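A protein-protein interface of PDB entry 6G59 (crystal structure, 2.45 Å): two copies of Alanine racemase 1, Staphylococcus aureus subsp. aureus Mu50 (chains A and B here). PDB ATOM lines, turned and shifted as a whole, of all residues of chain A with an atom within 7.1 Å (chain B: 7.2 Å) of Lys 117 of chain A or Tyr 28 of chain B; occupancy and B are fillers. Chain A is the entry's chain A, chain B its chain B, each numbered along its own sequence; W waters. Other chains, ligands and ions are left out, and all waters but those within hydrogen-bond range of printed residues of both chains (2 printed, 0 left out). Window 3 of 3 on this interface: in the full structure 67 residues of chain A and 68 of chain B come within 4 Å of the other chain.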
ATOM      1  N   THR A  88       0.430   5.240  37.192  1.00  0.00           N
ATOM      2  CA  THR A  88      -0.077   5.533  35.865  1.00  0.00           C
ATOM      3  C   THR A  88       1.051   6.051  34.987  1.00  0.00           C
ATOM      4  O   THR A  88       2.045   6.571  35.497  1.00  0.00           O
ATOM      5  CB  THR A  88      -1.169   6.632  35.940  1.00  0.00           C
ATOM      6  OG1 THR A  88      -0.552   7.918  36.129  1.00  0.00           O
ATOM      7  CG2 THR A  88      -2.167   6.371  37.097  1.00  0.00           C
ATOM      8  N   LEU A  89       0.884   5.937  33.669  1.00  0.00           N
ATOM      9  CA  LEU A  89       1.843   6.507  32.720  1.00  0.00           C
ATOM     10  C   LEU A  89       1.901   8.046  32.784  1.00  0.00           C
ATOM     11  O   LEU A  89       2.969   8.640  32.566  1.00  0.00           O
ATOM     12  CB  LEU A  89       1.535   6.040  31.290  1.00  0.00           C
ATOM     13  CG  LEU A  89       2.489   6.556  30.203  1.00  0.00           C
ATOM     14  CD1 LEU A  89       3.929   6.152  30.482  1.00  0.00           C
ATOM     15  CD2 LEU A  89       2.050   6.085  28.825  1.00  0.00           C
ATOM     16  N   ASP A  90       0.756   8.678  33.063  1.00  0.00           N
ATOM     17  CA  ASP A  90       0.707  10.138  33.248  1.00  0.00           C
ATOM     18  C   ASP A  90       1.716  10.558  34.330  1.00  0.00           C
ATOM     19  O   ASP A  90       2.478  11.494  34.135  1.00  0.00           O
ATOM     20  CB  ASP A  90      -0.690  10.627  33.667  1.00  0.00           C
ATOM     21  CG  ASP A  90      -1.805  10.143  32.737  1.00  0.00           C
ATOM     22  OD1 ASP A  90      -2.379   9.048  33.012  1.00  0.00           O
ATOM     23  OD2 ASP A  90      -2.118  10.862  31.745  1.00  0.00           O
ATOM     24  N   GLU A  91       1.694   9.858  35.466  1.00  0.00           N
ATOM     25  CA  GLU A  91       2.639  10.094  36.573  1.00  0.00           C
ATOM     26  C   GLU A  91       4.106   9.912  36.167  1.00  0.00           C
ATOM     27  O   GLU A  91       4.967  10.687  36.595  1.00  0.00           O
ATOM     28  CB  GLU A  91       2.316   9.186  37.781  1.00  0.00           C
ATOM     29  CG  GLU A  91       1.049   9.614  38.523  1.00  0.00           C
ATOM     30  CD  GLU A  91       0.603   8.664  39.623  1.00  0.00           C
ATOM     31  OE1 GLU A  91       1.116   7.520  39.702  1.00  0.00           O
ATOM     32  OE2 GLU A  91      -0.290   9.082  40.409  1.00  0.00           O
ATOM     33  N   ILE A  93       5.290  10.069  32.882  1.00  0.00           N
ATOM     34  CA  ILE A  93       5.595  11.152  31.937  1.00  0.00           C
ATOM     35  C   ILE A  93       5.822  12.487  32.673  1.00  0.00           C
ATOM     36  O   ILE A  93       6.719  13.229  32.309  1.00  0.00           O
ATOM     37  CB  ILE A  93       4.515  11.295  30.834  1.00  0.00           C
ATOM     38  CG1 ILE A  93       4.510  10.068  29.915  1.00  0.00           C
ATOM     39  CG2 ILE A  93       4.741  12.556  29.998  1.00  0.00           C
ATOM     40  CD1 ILE A  93       3.296   9.988  28.997  1.00  0.00           C
ATOM     41  N   VAL A 106       5.469   1.612  35.791  1.00  0.00           N
ATOM     42  CA  VAL A 106       4.050   1.853  35.949  1.00  0.00           C
ATOM     43  C   VAL A 106       3.440   0.565  36.500  1.00  0.00           C
ATOM     44  O   VAL A 106       3.521  -0.480  35.859  1.00  0.00           O
ATOM     45  CB  VAL A 106       3.382   2.278  34.608  1.00  0.00           C
ATOM     46  CG1 VAL A 106       1.868   2.400  34.758  1.00  0.00           C
ATOM     47  CG2 VAL A 106       3.958   3.607  34.124  1.00  0.00           C
ATOM     48  N   VAL A 109      -2.288  -0.798  34.775  1.00  0.00           N
ATOM     49  CA  VAL A 109      -2.420  -1.335  33.431  1.00  0.00           C
ATOM     50  C   VAL A 109      -2.577  -0.217  32.413  1.00  0.00           C
ATOM     51  O   VAL A 109      -3.556   0.520  32.438  1.00  0.00           O
ATOM     52  CB  VAL A 109      -3.643  -2.261  33.335  1.00  0.00           C
ATOM     53  CG1 VAL A 109      -3.773  -2.833  31.928  1.00  0.00           C
ATOM     54  CG2 VAL A 109      -3.523  -3.379  34.366  1.00  0.00           C
ATOM     55  N   LEU A 110      -1.608  -0.100  31.518  1.00  0.00           N
ATOM     56  CA  LEU A 110      -1.678   0.863  30.435  1.00  0.00           C
ATOM     57  C   LEU A 110      -2.724   0.420  29.401  1.00  0.00           C
ATOM     58  O   LEU A 110      -2.772  -0.755  29.044  1.00  0.00           O
ATOM     59  CB  LEU A 110      -0.313   0.970  29.755  1.00  0.00           C
ATOM     60  CG  LEU A 110      -0.184   2.056  28.693  1.00  0.00           C
ATOM     61  CD1 LEU A 110      -0.090   3.438  29.325  1.00  0.00           C
ATOM     62  CD2 LEU A 110       1.022   1.797  27.807  1.00  0.00           C
ATOM     63  N   PRO A 111      -3.558   1.358  28.912  1.00  0.00           N
ATOM     64  CA  PRO A 111      -4.331   1.098  27.688  1.00  0.00           C
ATOM     65  C   PRO A 111      -3.427   0.737  26.501  1.00  0.00           C
ATOM     66  O   PRO A 111      -2.485   1.459  26.200  1.00  0.00           O
ATOM     67  CB  PRO A 111      -5.061   2.430  27.424  1.00  0.00           C
ATOM     68  CG  PRO A 111      -5.066   3.155  28.713  1.00  0.00           C
ATOM     69  CD  PRO A 111      -3.896   2.658  29.519  1.00  0.00           C
ATOM     70  N   LYS A 113      -3.642   0.985  23.324  1.00  0.00           N
ATOM     71  CA  LYS A 113      -3.479   2.015  22.288  1.00  0.00           C
ATOM     72  C   LYS A 113      -2.329   3.008  22.590  1.00  0.00           C
ATOM     73  O   LYS A 113      -1.766   3.580  21.678  1.00  0.00           O
ATOM     74  CB  LYS A 113      -4.808   2.755  22.003  1.00  0.00           C
ATOM     75  CG  LYS A 113      -5.228   3.766  23.068  1.00  0.00           C
ATOM     76  CD  LYS A 113      -6.594   4.391  22.781  1.00  0.00           C
ATOM     77  CE  LYS A 113      -7.138   5.161  23.990  1.00  0.00           C
ATOM     78  NZ  LYS A 113      -6.483   6.474  24.248  1.00  0.00           N
ATOM     79  N   ASP A 114      -1.985   3.179  23.861  1.00  0.00           N
ATOM     80  CA  ASP A 114      -0.939   4.108  24.306  1.00  0.00           C
ATOM     81  C   ASP A 114       0.476   3.509  24.435  1.00  0.00           C
ATOM     82  O   ASP A 114       1.378   4.171  24.928  1.00  0.00           O
ATOM     83  CB  ASP A 114      -1.341   4.712  25.663  1.00  0.00           C
ATOM     84  CG  ASP A 114      -2.666   5.475  25.609  1.00  0.00           C
ATOM     85  OD1 ASP A 114      -3.070   6.001  24.542  1.00  0.00           O
ATOM     86  OD2 ASP A 114      -3.287   5.582  26.679  1.00  0.00           O
ATOM     87  N   ILE A 115       0.674   2.280  23.965  1.00  0.00           N
ATOM     88  CA  ILE A 115       1.963   1.585  24.080  1.00  0.00           C
ATOM     89  C   ILE A 115       3.165   2.380  23.514  1.00  0.00           C
ATOM     90  O   ILE A 115       4.227   2.396  24.127  1.00  0.00           O
ATOM     91  CB  ILE A 115       1.872   0.164  23.468  1.00  0.00           C
ATOM     92  CG1 ILE A 115       3.051  -0.714  23.913  1.00  0.00           C
ATOM     93  CG2 ILE A 115       1.782   0.197  21.943  1.00  0.00           C
ATOM     94  CD1 ILE A 115       2.949  -1.215  25.332  1.00  0.00           C
ATOM     95  N   ASP A 116       2.990   3.058  22.378  1.00  0.00           N
ATOM     96  CA  ASP A 116       4.073   3.876  21.785  1.00  0.00           C
ATOM     97  C   ASP A 116       4.599   5.021  22.682  1.00  0.00           C
ATOM     98  O   ASP A 116       5.785   5.339  22.630  1.00  0.00           O
ATOM     99  CB  ASP A 116       3.670   4.458  20.412  1.00  0.00           C
ATOM    100  CG  ASP A 116       3.789   3.452  19.263  1.00  0.00           C
ATOM    101  OD1 ASP A 116       4.436   2.387  19.408  1.00  0.00           O
ATOM    102  OD2 ASP A 116       3.242   3.755  18.191  1.00  0.00           O
ATOM    103  N   LYS A 117       3.731   5.621  23.492  1.00  0.00           N
ATOM    104  CA  LYS A 117       4.149   6.659  24.433  1.00  0.00           C
ATOM    105  C   LYS A 117       5.032   6.129  25.562  1.00  0.00           C
ATOM    106  O   LYS A 117       5.906   6.847  26.036  1.00  0.00           O
ATOM    107  CB  LYS A 117       2.943   7.392  25.028  1.00  0.00           C
ATOM    108  CG  LYS A 117       2.245   8.302  24.041  1.00  0.00           C
ATOM    109  CD  LYS A 117       2.992   9.615  23.827  1.00  0.00           C
ATOM    110  CE  LYS A 117       2.728  10.159  22.433  1.00  0.00           C
ATOM    111  NZ  LYS A 117       3.445  11.443  22.239  1.00  0.00           N
ATOM    112  N   ALA A 118       4.808   4.894  26.006  1.00  0.00           N
ATOM    113  CA  ALA A 118       5.676   4.275  27.023  1.00  0.00           C
ATOM    114  C   ALA A 118       7.073   3.992  26.476  1.00  0.00           C
ATOM    115  O   ALA A 118       8.072   4.213  27.152  1.00  0.00           O
ATOM    116  CB  ALA A 118       5.053   3.005  27.559  1.00  0.00           C
ATOM    117  N   ILE A 119       7.125   3.532  25.233  1.00  0.00           N
ATOM    118  CA  ILE A 119       8.390   3.248  24.562  1.00  0.00           C
ATOM    119  C   ILE A 119       9.160   4.535  24.329  1.00  0.00           C
ATOM    120  O   ILE A 119      10.347   4.603  24.641  1.00  0.00           O
ATOM    121  CB  ILE A 119       8.181   2.518  23.224  1.00  0.00           C
ATOM    122  CG1 ILE A 119       7.545   1.144  23.461  1.00  0.00           C
ATOM    123  CG2 ILE A 119       9.510   2.364  22.499  1.00  0.00           C
ATOM    124  CD1 ILE A 119       6.983   0.488  22.227  1.00  0.00           C
ATOM    125  N   GLN A 120       8.482   5.541  23.788  1.00  0.00           N
ATOM    126  CA  GLN A 120       9.093   6.859  23.545  1.00  0.00           C
ATOM    127  C   GLN A 120       9.759   7.443  24.783  1.00  0.00           C
ATOM    128  O   GLN A 120      10.900   7.894  24.706  1.00  0.00           O
ATOM    129  CB  GLN A 120       8.055   7.853  23.022  1.00  0.00           C
ATOM    130  CG  GLN A 120       8.629   9.169  22.528  1.00  0.00           C
ATOM    131  CD  GLN A 120       7.581  10.068  21.899  1.00  0.00           C
ATOM    132  OE1 GLN A 120       6.471  10.245  22.430  1.00  0.00           O
ATOM    133  NE2 GLN A 120       7.926  10.642  20.755  1.00  0.00           N
ATOM    134  N   HIS A 121       9.046   7.417  25.915  1.00  0.00           N
ATOM    135  CA  HIS A 121       9.545   7.989  27.171  1.00  0.00           C
ATOM    136  C   HIS A 121      10.328   7.040  28.073  1.00  0.00           C
ATOM    137  O   HIS A 121      10.613   7.400  29.205  1.00  0.00           O
ATOM    138  CB  HIS A 121       8.404   8.616  27.979  1.00  0.00           C
ATOM    139  CG  HIS A 121       7.851   9.856  27.368  1.00  0.00           C
ATOM    140  ND1 HIS A 121       8.496  11.076  27.433  1.00  0.00           N
ATOM    141  CD2 HIS A 121       6.712  10.067  26.672  1.00  0.00           C
ATOM    142  CE1 HIS A 121       7.774  11.980  26.798  1.00  0.00           C
ATOM    143  NE2 HIS A 121       6.688  11.393  26.328  1.00  0.00           N
ATOM    144  N   ARG A 122      10.665   5.843  27.610  1.00  0.00           N
ATOM    145  CA  ARG A 122      11.570   4.951  28.363  1.00  0.00           C
ATOM    146  C   ARG A 122      11.034   4.547  29.735  1.00  0.00           C
ATOM    147  O   ARG A 122      11.746   4.579  30.737  1.00  0.00           O
ATOM    148  CB  ARG A 122      12.977   5.582  28.470  1.00  0.00           C
ATOM    149  CG  ARG A 122      13.583   5.902  27.107  1.00  0.00           C
ATOM    150  CD  ARG A 122      13.814   4.606  26.323  1.00  0.00           C
ATOM    151  NE  ARG A 122      15.230   4.268  26.173  1.00  0.00           N
ATOM    152  CZ  ARG A 122      15.718   3.033  26.032  1.00  0.00           C
ATOM    153  NH1 ARG A 122      14.919   1.946  26.031  1.00  0.00           N
ATOM    154  NH2 ARG A 122      17.039   2.889  25.904  1.00  0.00           N
ATOM    155  N   VAL A 123       9.764   4.152  29.738  1.00  0.00           N
ATOM    156  CA  VAL A 123       9.018   3.806  30.929  1.00  0.00           C
ATOM    157  C   VAL A 123       8.677   2.326  30.889  1.00  0.00           C
ATOM    158  O   VAL A 123       8.143   1.832  29.898  1.00  0.00           O
ATOM    159  CB  VAL A 123       7.720   4.615  30.991  1.00  0.00           C
ATOM    160  CG1 VAL A 123       6.877   4.212  32.194  1.00  0.00           C
ATOM    161  CG2 VAL A 123       8.042   6.106  31.022  1.00  0.00           C
ATOM    162  N   GLN A 144       8.369   4.204  17.174  1.00  0.00           N
ATOM    163  CA  GLN A 144       9.263   4.223  18.339  1.00  0.00           C
ATOM    164  C   GLN A 144       9.993   2.872  18.386  1.00  0.00           C
ATOM    165  O   GLN A 144       9.377   1.855  18.700  1.00  0.00           O
ATOM    166  CB  GLN A 144       8.448   4.457  19.617  1.00  0.00           C
ATOM    167  CG  GLN A 144       7.567   5.702  19.580  1.00  0.00           C
ATOM    168  CD  GLN A 144       8.374   7.002  19.475  1.00  0.00           C
ATOM    169  OE1 GLN A 144       9.488   7.092  19.979  1.00  0.00           O
ATOM    170  NE2 GLN A 144       7.803   8.012  18.842  1.00  0.00           N
ATOM    171  N   PHE B  23       1.506  18.438  27.614  1.00  0.00           N
ATOM    172  CA  PHE B  23       0.604  17.478  26.951  1.00  0.00           C
ATOM    173  C   PHE B  23      -0.714  17.380  27.745  1.00  0.00           C
ATOM    174  O   PHE B  23      -1.281  16.288  27.883  1.00  0.00           O
ATOM    175  CB  PHE B  23       1.238  16.099  26.875  1.00  0.00           C
ATOM    176  CG  PHE B  23       2.657  16.092  26.404  1.00  0.00           C
ATOM    177  CD1 PHE B  23       2.960  16.013  25.046  1.00  0.00           C
ATOM    178  CD2 PHE B  23       3.697  16.082  27.326  1.00  0.00           C
ATOM    179  CE1 PHE B  23       4.284  15.955  24.616  1.00  0.00           C
ATOM    180  CE2 PHE B  23       5.024  16.019  26.907  1.00  0.00           C
ATOM    181  CZ  PHE B  23       5.318  15.959  25.550  1.00  0.00           C
ATOM    182  N   LYS B  26      -3.734  15.472  26.567  1.00  0.00           N
ATOM    183  CA  LYS B  26      -3.664  14.017  26.488  1.00  0.00           C
ATOM    184  C   LYS B  26      -3.838  13.400  27.872  1.00  0.00           C
ATOM    185  O   LYS B  26      -3.617  14.057  28.890  1.00  0.00           O
ATOM    186  CB  LYS B  26      -2.336  13.556  25.857  1.00  0.00           C
ATOM    187  CG  LYS B  26      -2.299  13.832  24.360  1.00  0.00           C
ATOM    188  CD  LYS B  26      -3.265  12.903  23.616  1.00  0.00           C
ATOM    189  CE  LYS B  26      -3.071  12.954  22.095  1.00  0.00           C
ATOM    190  NZ  LYS B  26      -3.228  14.347  21.580  1.00  0.00           N
ATOM    191  N   TYR B  27      -4.262  12.136  27.892  1.00  0.00           N
ATOM    192  CA  TYR B  27      -4.319  11.359  29.121  1.00  0.00           C
ATOM    193  C   TYR B  27      -4.198   9.860  28.870  1.00  0.00           C
ATOM    194  O   TYR B  27      -4.673   9.357  27.864  1.00  0.00           O
ATOM    195  CB  TYR B  27      -5.582  11.682  29.916  1.00  0.00           C
ATOM    196  CG  TYR B  27      -6.825  11.077  29.351  1.00  0.00           C
ATOM    197  CD1 TYR B  27      -7.486  11.678  28.290  1.00  0.00           C
ATOM    198  CD2 TYR B  27      -7.352   9.904  29.880  1.00  0.00           C
ATOM    199  CE1 TYR B  27      -8.649  11.130  27.769  1.00  0.00           C
ATOM    200  CE2 TYR B  27      -8.514   9.346  29.369  1.00  0.00           C
ATOM    201  CZ  TYR B  27      -9.164   9.971  28.322  1.00  0.00           C
ATOM    202  OH  TYR B  27     -10.312   9.434  27.823  1.00  0.00           O
ATOM    203  N   TYR B  28      -3.593   9.152  29.823  1.00  0.00           N
ATOM    204  CA  TYR B  28      -3.067   7.809  29.593  1.00  0.00           C
ATOM    205  C   TYR B  28      -3.555   6.747  30.606  1.00  0.00           C
ATOM    206  O   TYR B  28      -2.898   5.714  30.808  1.00  0.00           O
ATOM    207  CB  TYR B  28      -1.522   7.886  29.534  1.00  0.00           C
ATOM    208  CG  TYR B  28      -1.020   8.751  28.395  1.00  0.00           C
ATOM    209  CD1 TYR B  28      -1.109   8.313  27.081  1.00  0.00           C
ATOM    210  CD2 TYR B  28      -0.490  10.026  28.625  1.00  0.00           C
ATOM    211  CE1 TYR B  28      -0.698   9.110  26.025  1.00  0.00           C
ATOM    212  CE2 TYR B  28      -0.056  10.833  27.574  1.00  0.00           C
ATOM    213  CZ  TYR B  28      -0.170  10.375  26.274  1.00  0.00           C
ATOM    214  OH  TYR B  28       0.247  11.129  25.212  1.00  0.00           O
ATOM    215  N   ARG B  29      -4.695   7.007  31.241  1.00  0.00           N
ATOM    216  CA  ARG B  29      -5.386   6.008  32.049  1.00  0.00           C
ATOM    217  C   ARG B  29      -6.880   6.164  31.798  1.00  0.00           C
ATOM    218  O   ARG B  29      -7.367   7.290  31.716  1.00  0.00           O
ATOM    219  CB  ARG B  29      -5.062   6.203  33.540  1.00  0.00           C
ATOM    220  CG  ARG B  29      -5.784   5.237  34.480  1.00  0.00           C
ATOM    221  CD  ARG B  29      -5.564   5.562  35.943  1.00  0.00           C
ATOM    222  NE  ARG B  29      -6.132   6.866  36.278  1.00  0.00           N
ATOM    223  CZ  ARG B  29      -6.425   7.312  37.499  1.00  0.00           C
ATOM    224  NH1 ARG B  29      -6.243   6.569  38.580  1.00  0.00           N
ATOM    225  NH2 ARG B  29      -6.935   8.539  37.623  1.00  0.00           N
ATOM    226  N   SER B  30      -7.605   5.047  31.701  1.00  0.00           N
ATOM    227  CA  SER B  30      -9.045   5.072  31.391  1.00  0.00           C
ATOM    228  C   SER B  30      -9.908   5.347  32.615  1.00  0.00           C
ATOM    229  O   SER B  30     -10.664   4.487  33.075  1.00  0.00           O
ATOM    230  CB  SER B  30      -9.476   3.756  30.745  1.00  0.00           C
ATOM    231  OG  SER B  30      -8.748   3.521  29.554  1.00  0.00           O
ATOM    232  N   ALA B  31      -9.789   6.562  33.134  1.00  0.00           N
ATOM    233  CA  ALA B  31     -10.579   7.022  34.276  1.00  0.00           C
ATOM    234  C   ALA B  31     -10.583   8.525  34.188  1.00  0.00           C
ATOM    235  O   ALA B  31      -9.525   9.121  34.022  1.00  0.00           O
ATOM    236  CB  ALA B  31      -9.974   6.561  35.595  1.00  0.00           C
ATOM    237  N   PRO B 387      -8.405  13.378  34.817  1.00  0.00           N
ATOM    238  CA  PRO B 387      -8.635  14.348  33.746  1.00  0.00           C
ATOM    239  C   PRO B 387     -10.057  14.865  33.735  1.00  0.00           C
ATOM    240  O   PRO B 387     -10.978  14.111  34.076  1.00  0.00           O
ATOM    241  CB  PRO B 387      -8.385  13.524  32.472  1.00  0.00           C
ATOM    242  CG  PRO B 387      -7.534  12.382  32.922  1.00  0.00           C
ATOM    243  CD  PRO B 387      -8.061  12.054  34.272  1.00  0.00           C
ATOM    244  N   ASN B 400      -5.591  17.628  31.787  1.00  0.00           N
ATOM    245  CA  ASN B 400      -4.925  16.653  32.655  1.00  0.00           C
ATOM    246  C   ASN B 400      -3.803  17.435  33.357  1.00  0.00           C
ATOM    247  O   ASN B 400      -2.760  17.730  32.767  1.00  0.00           O
ATOM    248  CB  ASN B 400      -4.371  15.513  31.812  1.00  0.00           C
ATOM    249  CG  ASN B 400      -3.629  14.460  32.621  1.00  0.00           C
ATOM    250  OD1 ASN B 400      -3.535  14.520  33.850  1.00  0.00           O
ATOM    251  ND2 ASN B 400      -3.078  13.488  31.902  1.00  0.00           N
ATOM    252  N   LEU B 403       0.178  16.772  33.351  1.00  0.00           N
ATOM    253  CA  LEU B 403       0.976  17.025  32.166  1.00  0.00           C
ATOM    254  C   LEU B 403       1.024  18.521  31.746  1.00  0.00           C
ATOM    255  O   LEU B 403       1.386  18.827  30.604  1.00  0.00           O
ATOM    256  CB  LEU B 403       0.480  16.123  31.039  1.00  0.00           C
ATOM    257  CG  LEU B 403       0.388  14.627  31.383  1.00  0.00           C
ATOM    258  CD1 LEU B 403      -0.103  13.842  30.167  1.00  0.00           C
ATOM    259  CD2 LEU B 403       1.700  14.029  31.890  1.00  0.00           C
HETATM  260  O   HOH W   1      -1.694   4.458  32.868  1.00  0.00           O
HETATM  261  O   HOH W   2      -6.393   2.240  32.194  1.00  0.00           O
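Water W1 bridges the backbone carbonyl oxygen (O) of Tyr 28 of chain B (2.7 Å) and the backbone NH (N) of Leu 89 of chain A (3.1 Å).
Water W2 lies within hydrogen-bond range of the backbone NH of Ser 30 of chain B and the backbone carbonyl oxygen of Val 109 of chain A.
No position is printed for both chains.
Among the printed residues, pairs that only touch across the chains: Thr 88 of chain A with Arg 29 of chain B (3.7 Å), Leu 89 of chain A with Tyr 28 of chain B (3.98 Å), Asp 90 of chain A with Tyr 27 of chain B (3.5 Å), Asp 90 of chain A with Arg 29 of chain B (3.6 Å), Asp 90 of chain A with Leu 403 of chain B (3.5 Å), Ile 93 of chain A with Tyr 28 of chain B (3.7 Å), Ile 93 of chain A with Leu 403 of chain B (3.9 Å), Leu 110 of chain A with Tyr 28 of chain B (3.9 Å), Pro 111 of chain A with Tyr 28 of chain B (3.5 Å), Pro 111 of chain A with Ser 30 of chain B (3.8 Å), Asp 114 of chain A with Tyr 28 of chain B (3.5 Å) and Lys 117 of chain A with Tyr 28 of chain B (3.4 Å).
The backbone carbonyl oxygen of Lys 26 of chain B is in hydrogen-bond range of the side-chain amide nitrogen of Asn 400 of chain B (3.1 Å).
The side-chain amino group (NZ) of Lys 113 of chain A is in salt-bridge range of the side-chain carboxylate (OD1) of Asp 114 of chain A (3.5 Å).
The side-chain amino group (NZ) of Lys 117 of chain A is in hydrogen-bond range of the side-chain amide oxygen (OE1) of Gln 120 of chain A (3.3 Å).
N of Phe 23 of chain B lies within hydrogen-bond range of O of Leu 403 of chain B, 3.0 Å away.
The side-chain hydroxyl (OG1) of Thr 88 of chain A sits at hydrogen-bond distance from the backbone NH (N) of Glu 91 of chain A (3.0 Å).
The backbone NH (N) of Asp 90 of chain A sits close to the side-chain hydroxyl (OG1) of Thr 88 of chain A (3.4 Å).
Printed residues of chain A that touch a printed residue of chain B: Thr 88, Leu 89, Asp 90, Ile 93, Leu 110, Pro 111, Asp 114 and Lys 117.
Among the printed residues, 14 pairs touch across the chains.
Among the printed residues, no Asp or Glu carboxylate lies within 4 Å of a Lys or Arg side-chain nitrogen of the other chain.
Of chain A, only Leu 89 (3.98 Å), Asp 90 (3.0 Å), Ile 93 (3.7 Å), Leu 110 (3.9 Å), Pro 111 (3.5 Å), Asp 114 (3.5 Å) and Lys 117 (3.4 Å) come within 4 Å of Tyr 28 of chain B.
Printed residues of chain B within 4 Å of Asp 90 of chain A: Tyr 27, Tyr 28, Arg 29, Asn 400 and Leu 403.
Of the printed residues of chain A, Arg 29 of chain B touches Thr 88 (3.7 Å) and Asp 90 (3.6 Å).
Glu 91 of chain A touches none of the printed residues of chain B.
Ile 119 of chain A touches none of the printed residues of chain B.
The nearest residue of chain B that does not touch Lys 117 of chain A is Phe 23 of chain B (5.2 Å).
The nearest printed residue of chain A that does not touch Tyr 28 of chain B is Val 109 of chain A (5.5 Å).
The side-chain carboxylate of Asp 90 of chain A sits at hydrogen-bond distance from the side-chain amide nitrogen of Asn 400 of chain B.
OD2 of Asp 90 of chain A lies within hydrogen-bond range of N of Tyr 28 of chain B (3.0 Å).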
